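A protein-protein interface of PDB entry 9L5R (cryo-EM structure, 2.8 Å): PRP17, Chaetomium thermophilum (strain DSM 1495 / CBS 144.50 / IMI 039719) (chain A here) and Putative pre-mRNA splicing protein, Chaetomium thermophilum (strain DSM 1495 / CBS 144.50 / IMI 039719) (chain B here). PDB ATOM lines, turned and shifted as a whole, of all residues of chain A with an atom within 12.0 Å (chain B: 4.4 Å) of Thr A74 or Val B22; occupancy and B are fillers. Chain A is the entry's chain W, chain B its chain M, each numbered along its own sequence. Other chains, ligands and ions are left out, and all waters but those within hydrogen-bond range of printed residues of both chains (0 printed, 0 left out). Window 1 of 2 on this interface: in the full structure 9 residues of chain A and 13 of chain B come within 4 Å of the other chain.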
ATOM      1  N   LYS A  69      12.125 -36.032  23.100  1.00  0.00           N
ATOM      2  CA  LYS A  69      12.710 -36.456  21.835  1.00  0.00           C
ATOM      3  C   LYS A  69      13.543 -35.325  21.235  1.00  0.00           C
ATOM      4  O   LYS A  69      13.036 -34.486  20.489  1.00  0.00           O
ATOM      5  CB  LYS A  69      11.616 -36.908  20.868  1.00  0.00           C
ATOM      6  CG  LYS A  69      10.807 -38.104  21.376  1.00  0.00           C
ATOM      7  CD  LYS A  69       9.910 -38.679  20.295  1.00  0.00           C
ATOM      8  CE  LYS A  69       8.709 -37.788  20.030  1.00  0.00           C
ATOM      9  NZ  LYS A  69       7.787 -38.380  19.025  1.00  0.00           N
ATOM     10  N   ASN A  70      14.832 -35.325  21.572  1.00  0.00           N
ATOM     11  CA  ASN A  70      15.721 -34.226  21.226  1.00  0.00           C
ATOM     12  C   ASN A  70      16.007 -34.192  19.731  1.00  0.00           C
ATOM     13  O   ASN A  70      16.272 -35.225  19.111  1.00  0.00           O
ATOM     14  CB  ASN A  70      17.031 -34.351  21.997  1.00  0.00           C
ATOM     15  CG  ASN A  70      16.891 -33.976  23.452  1.00  0.00           C
ATOM     16  OD1 ASN A  70      17.849 -34.054  24.216  1.00  0.00           O
ATOM     17  ND2 ASN A  70      15.699 -33.550  23.841  1.00  0.00           N
ATOM     18  N   ASN A  71      15.958 -32.996  19.155  1.00  0.00           N
ATOM     19  CA  ASN A  71      16.341 -32.793  17.767  1.00  0.00           C
ATOM     20  C   ASN A  71      17.757 -32.252  17.612  1.00  0.00           C
ATOM     21  O   ASN A  71      18.354 -32.403  16.539  1.00  0.00           O
ATOM     22  CB  ASN A  71      15.315 -31.883  17.077  1.00  0.00           C
ATOM     23  CG  ASN A  71      15.181 -30.513  17.736  1.00  0.00           C
ATOM     24  OD1 ASN A  71      15.907 -30.163  18.662  1.00  0.00           O
ATOM     25  ND2 ASN A  71      14.238 -29.729  17.243  1.00  0.00           N
ATOM     26  N   VAL A  72      18.299 -31.640  18.650  1.00  0.00           N
ATOM     27  CA  VAL A  72      19.696 -31.239  18.713  1.00  0.00           C
ATOM     28  C   VAL A  72      20.434 -32.316  19.494  1.00  0.00           C
ATOM     29  O   VAL A  72      19.856 -32.989  20.350  1.00  0.00           O
ATOM     30  CB  VAL A  72      19.814 -29.827  19.344  1.00  0.00           C
ATOM     31  CG1 VAL A  72      21.251 -29.406  19.635  1.00  0.00           C
ATOM     32  CG2 VAL A  72      19.183 -28.820  18.426  1.00  0.00           C
ATOM     33  N   LEU A  73      21.707 -32.527  19.160  1.00  0.00           N
ATOM     34  CA  LEU A  73      22.504 -33.562  19.803  1.00  0.00           C
ATOM     35  C   LEU A  73      22.761 -33.282  21.279  1.00  0.00           C
ATOM     36  O   LEU A  73      23.136 -34.201  22.011  1.00  0.00           O
ATOM     37  CB  LEU A  73      23.830 -33.703  19.063  1.00  0.00           C
ATOM     38  CG  LEU A  73      24.558 -35.036  19.050  1.00  0.00           C
ATOM     39  CD1 LEU A  73      23.678 -36.079  18.408  1.00  0.00           C
ATOM     40  CD2 LEU A  73      25.852 -34.875  18.279  1.00  0.00           C
ATOM     41  N   THR A  74      22.564 -32.044  21.732  1.00  0.00           N
ATOM     42  CA  THR A  74      22.835 -31.656  23.110  1.00  0.00           C
ATOM     43  C   THR A  74      21.597 -31.166  23.847  1.00  0.00           C
ATOM     44  O   THR A  74      21.727 -30.608  24.939  1.00  0.00           O
ATOM     45  CB  THR A  74      23.905 -30.564  23.152  1.00  0.00           C
ATOM     46  OG1 THR A  74      23.520 -29.492  22.284  1.00  0.00           O
ATOM     47  CG2 THR A  74      25.226 -31.103  22.700  1.00  0.00           C
ATOM     48  N   GLY A  75      20.415 -31.337  23.288  1.00  0.00           N
ATOM     49  CA  GLY A  75      19.224 -30.817  23.911  1.00  0.00           C
ATOM     50  C   GLY A  75      18.119 -30.641  22.897  1.00  0.00           C
ATOM     51  O   GLY A  75      18.170 -31.183  21.804  1.00  0.00           O
ATOM     52  N   HIS A  76      17.108 -29.879  23.296  1.00  0.00           N
ATOM     53  CA  HIS A  76      15.971 -29.578  22.442  1.00  0.00           C
ATOM     54  C   HIS A  76      15.959 -28.088  22.144  1.00  0.00           C
ATOM     55  O   HIS A  76      15.968 -27.270  23.065  1.00  0.00           O
ATOM     56  CB  HIS A  76      14.658 -29.998  23.103  1.00  0.00           C
ATOM     57  CG  HIS A  76      13.473 -29.892  22.201  1.00  0.00           C
ATOM     58  ND1 HIS A  76      13.357 -30.624  21.040  1.00  0.00           N
ATOM     59  CD2 HIS A  76      12.354 -29.138  22.284  1.00  0.00           C
ATOM     60  CE1 HIS A  76      12.218 -30.325  20.446  1.00  0.00           C
ATOM     61  NE2 HIS A  76      11.591 -29.424  21.179  1.00  0.00           N
ATOM     62  N   ALA A  77      15.944 -27.743  20.859  1.00  0.00           N
ATOM     63  CA  ALA A  77      15.894 -26.359  20.411  1.00  0.00           C
ATOM     64  C   ALA A  77      14.598 -26.119  19.654  1.00  0.00           C
ATOM     65  O   ALA A  77      14.240 -26.898  18.768  1.00  0.00           O
ATOM     66  CB  ALA A  77      17.084 -26.022  19.522  1.00  0.00           C
ATOM     67  N   GLU A  78      13.907 -25.040  19.998  1.00  0.00           N
ATOM     68  CA  GLU A  78      12.634 -24.709  19.381  1.00  0.00           C
ATOM     69  C   GLU A  78      12.657 -23.248  18.961  1.00  0.00           C
ATOM     70  O   GLU A  78      13.167 -22.397  19.692  1.00  0.00           O
ATOM     71  CB  GLU A  78      11.486 -24.985  20.358  1.00  0.00           C
ATOM     72  CG  GLU A  78      10.099 -24.765  19.818  1.00  0.00           C
ATOM     73  CD  GLU A  78       9.037 -25.114  20.839  1.00  0.00           C
ATOM     74  OE1 GLU A  78       9.406 -25.501  21.966  1.00  0.00           O
ATOM     75  OE2 GLU A  78       7.836 -25.017  20.513  1.00  0.00           O
ATOM     76  N   PRO B  20      23.582 -24.984  16.679  1.00  0.00           N
ATOM     77  CA  PRO B  20      24.782 -25.759  16.987  1.00  0.00           C
ATOM     78  C   PRO B  20      24.574 -26.765  18.108  1.00  0.00           C
ATOM     79  O   PRO B  20      23.698 -26.627  18.960  1.00  0.00           O
ATOM     80  CB  PRO B  20      25.782 -24.679  17.400  1.00  0.00           C
ATOM     81  CG  PRO B  20      24.947 -23.604  17.918  1.00  0.00           C
ATOM     82  CD  PRO B  20      23.785 -23.565  16.994  1.00  0.00           C
ATOM     83  N   SER B  21      25.410 -27.800  18.095  1.00  0.00           N
ATOM     84  CA  SER B  21      25.447 -28.785  19.172  1.00  0.00           C
ATOM     85  C   SER B  21      26.636 -28.466  20.069  1.00  0.00           C
ATOM     86  O   SER B  21      27.692 -29.079  19.994  1.00  0.00           O
ATOM     87  CB  SER B  21      25.520 -30.191  18.610  1.00  0.00           C
ATOM     88  OG  SER B  21      24.242 -30.614  18.191  1.00  0.00           O
ATOM     89  N   VAL B  22      26.434 -27.498  20.950  1.00  0.00           N
ATOM     90  CA  VAL B  22      27.475 -27.002  21.835  1.00  0.00           C
ATOM     91  C   VAL B  22      27.076 -27.302  23.269  1.00  0.00           C
ATOM     92  O   VAL B  22      25.913 -27.134  23.647  1.00  0.00           O
ATOM     93  CB  VAL B  22      27.712 -25.493  21.630  1.00  0.00           C
ATOM     94  CG1 VAL B  22      28.863 -25.031  22.456  1.00  0.00           C
ATOM     95  CG2 VAL B  22      28.005 -25.216  20.189  1.00  0.00           C
ATOM     96  N   CYS B  23      28.035 -27.764  24.058  1.00  0.00           N
ATOM     97  CA  CYS B  23      27.765 -28.152  25.429  1.00  0.00           C
ATOM     98  C   CYS B  23      27.676 -26.935  26.342  1.00  0.00           C
ATOM     99  O   CYS B  23      28.059 -25.822  25.981  1.00  0.00           O
ATOM    100  CB  CYS B  23      28.846 -29.097  25.926  1.00  0.00           C
ATOM    101  SG  CYS B  23      30.469 -28.358  26.160  1.00  0.00           S
ATOM    102  N   GLU B  24      27.175 -27.170  27.555  1.00  0.00           N
ATOM    103  CA  GLU B  24      26.840 -26.080  28.462  1.00  0.00           C
ATOM    104  C   GLU B  24      28.059 -25.405  29.070  1.00  0.00           C
ATOM    105  O   GLU B  24      27.954 -24.259  29.513  1.00  0.00           O
ATOM    106  CB  GLU B  24      25.925 -26.588  29.570  1.00  0.00           C
ATOM    107  CG  GLU B  24      24.617 -27.124  29.050  1.00  0.00           C
ATOM    108  CD  GLU B  24      23.896 -26.116  28.188  1.00  0.00           C
ATOM    109  OE1 GLU B  24      23.704 -24.976  28.651  1.00  0.00           O
ATOM    110  OE2 GLU B  24      23.532 -26.452  27.045  1.00  0.00           O
ATOM    111  N   CYS B  26      30.890 -24.923  27.265  1.00  0.00           N
ATOM    112  CA  CYS B  26      31.334 -24.066  26.176  1.00  0.00           C
ATOM    113  C   CYS B  26      30.371 -22.908  25.948  1.00  0.00           C
ATOM    114  O   CYS B  26      30.792 -21.835  25.509  1.00  0.00           O
ATOM    115  CB  CYS B  26      31.502 -24.887  24.898  1.00  0.00           C
ATOM    116  SG  CYS B  26      33.003 -25.896  24.795  1.00  0.00           S
ATOM    117  N   LEU B  27      29.090 -23.101  26.246  1.00  0.00           N
ATOM    118  CA  LEU B  27      28.120 -22.020  26.204  1.00  0.00           C
ATOM    119  C   LEU B  27      28.387 -21.029  27.339  1.00  0.00           C
ATOM    120  O   LEU B  27      29.022 -21.375  28.335  1.00  0.00           O
ATOM    121  CB  LEU B  27      26.708 -22.593  26.297  1.00  0.00           C
ATOM    122  CG  LEU B  27      26.122 -23.140  24.997  1.00  0.00           C
ATOM    123  CD1 LEU B  27      24.672 -23.526  25.176  1.00  0.00           C
ATOM    124  CD2 LEU B  27      26.258 -22.130  23.884  1.00  0.00           C
ATOM    125  N   TRP B  56      30.106 -17.065  19.736  1.00  0.00           N
ATOM    126  CA  TRP B  56      29.497 -16.299  20.807  1.00  0.00           C
ATOM    127  C   TRP B  56      30.586 -15.654  21.644  1.00  0.00           C
ATOM    128  O   TRP B  56      31.640 -16.243  21.884  1.00  0.00           O
ATOM    129  CB  TRP B  56      28.586 -17.175  21.685  1.00  0.00           C
ATOM    130  CG  TRP B  56      29.235 -18.433  22.137  1.00  0.00           C
ATOM    131  CD1 TRP B  56      29.845 -18.647  23.328  1.00  0.00           C
ATOM    132  CD2 TRP B  56      29.351 -19.650  21.401  1.00  0.00           C
ATOM    133  NE1 TRP B  56      30.338 -19.916  23.382  1.00  0.00           N
ATOM    134  CE2 TRP B  56      30.053 -20.553  22.204  1.00  0.00           C
ATOM    135  CE3 TRP B  56      28.937 -20.058  20.133  1.00  0.00           C
ATOM    136  CZ2 TRP B  56      30.342 -21.842  21.791  1.00  0.00           C
ATOM    137  CZ3 TRP B  56      29.232 -21.335  19.721  1.00  0.00           C
ATOM    138  CH2 TRP B  56      29.929 -22.210  20.544  1.00  0.00           C
ATOM    139  N   THR B  69      32.006 -22.802  16.935  1.00  0.00           N
ATOM    140  CA  THR B  69      32.003 -24.185  16.497  1.00  0.00           C
ATOM    141  C   THR B  69      33.187 -24.427  15.572  1.00  0.00           C
ATOM    142  O   THR B  69      33.446 -23.643  14.657  1.00  0.00           O
ATOM    143  CB  THR B  69      30.693 -24.519  15.794  1.00  0.00           C
ATOM    144  OG1 THR B  69      30.631 -23.856  14.531  1.00  0.00           O
ATOM    145  CG2 THR B  69      29.524 -24.103  16.637  1.00  0.00           C
ATOM    146  N   CYS B  82      31.184 -32.499  21.220  1.00  0.00           N
ATOM    147  CA  CYS B  82      30.756 -31.112  21.256  1.00  0.00           C
ATOM    148  C   CYS B  82      31.376 -30.375  20.087  1.00  0.00           C
ATOM    149  O   CYS B  82      32.503 -30.646  19.677  1.00  0.00           O
ATOM    150  CB  CYS B  82      31.143 -30.408  22.552  1.00  0.00           C
ATOM    151  SG  CYS B  82      30.986 -28.595  22.435  1.00  0.00           S
ATOM    152  N   CYS B  84      32.218 -27.223  19.742  1.00  0.00           N
ATOM    153  CA  CYS B  84      33.280 -26.281  20.079  1.00  0.00           C
ATOM    154  C   CYS B  84      34.517 -26.975  20.645  1.00  0.00           C
ATOM    155  O   CYS B  84      35.609 -26.860  20.087  1.00  0.00           O
ATOM    156  CB  CYS B  84      32.768 -25.240  21.080  1.00  0.00           C
ATOM    157  SG  CYS B  84      34.057 -24.193  21.800  1.00  0.00           S
ATOM    158  N   LEU B  89      30.425 -36.203  24.087  1.00  0.00           N
ATOM    159  CA  LEU B  89      29.227 -35.670  24.720  1.00  0.00           C
ATOM    160  C   LEU B  89      28.700 -36.535  25.852  1.00  0.00           C
ATOM    161  O   LEU B  89      27.747 -36.126  26.519  1.00  0.00           O
ATOM    162  CB  LEU B  89      28.121 -35.480  23.686  1.00  0.00           C
ATOM    163  CG  LEU B  89      28.225 -34.251  22.788  1.00  0.00           C
ATOM    164  CD1 LEU B  89      27.046 -34.186  21.855  1.00  0.00           C
ATOM    165  CD2 LEU B  89      28.310 -33.006  23.623  1.00  0.00           C
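The side-chain hydroxyl of Ser B21 sits close to the backbone NH of Leu A73 (3.3 Å).
O of Pro B20 touches CG1 of Val A72 (3.8 Å).
Ser B21 touches Val A72 (OG to CG1, 3.5 Å).
Leu B89 touches Leu A73 (CD1 to CD2, 3.8 Å).
Ser B21 touches Thr A74 (CA to OG1, 3.7 Å).
OG1 of Thr A74 touches O of Val B22, at 3.6 Å.
Thr A74 touches Leu B89.
Val B22 touches just one residue of chain A: Thr A74 (3.6 Å).
Pro B20 touches just one residue of chain A: Val A72 (3.8 Å).
No residue of chain A comes within 4 Å of Glu B24.
Thr B69 touches none of the printed residues of chain A.
No residue of chain A comes within 4 Å of Cys B82.
No residue of chain A comes within 4 Å of Cys B84.
Leu B89 touches just these residues of chain A: Leu A73 (3.8 Å) and Thr A74 (3.7 Å).
Of the printed residues of chain B, Val A72 touches Pro B20 and Ser B21.
Of the printed residues of chain B, Leu A73 touches Ser B21 and Leu B89.
Trp B56 touches none of the printed residues of chain A.
Asn A71 touches none of the printed residues of chain B.
The nearest residue of chain A that does not touch Val B22 is Val A72 (5.7 Å).
Printed residues of chain B that touch a printed residue of chain A: Pro B20, Ser B21, Val B22 and Leu B89.
Along chain B the printed residues that touch a printed residue of chain A span positions 20 to 89.
Hydrophobic or aromatic side chains of chain A that line the printed part of chain B: Val A72 and Leu A73.
Among the printed residues, 7 pairs touch across the chains.
Among the printed residues, no Asp or Glu carboxylate lies within 4 Å of a Lys or Arg side-chain nitrogen of the other chain.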
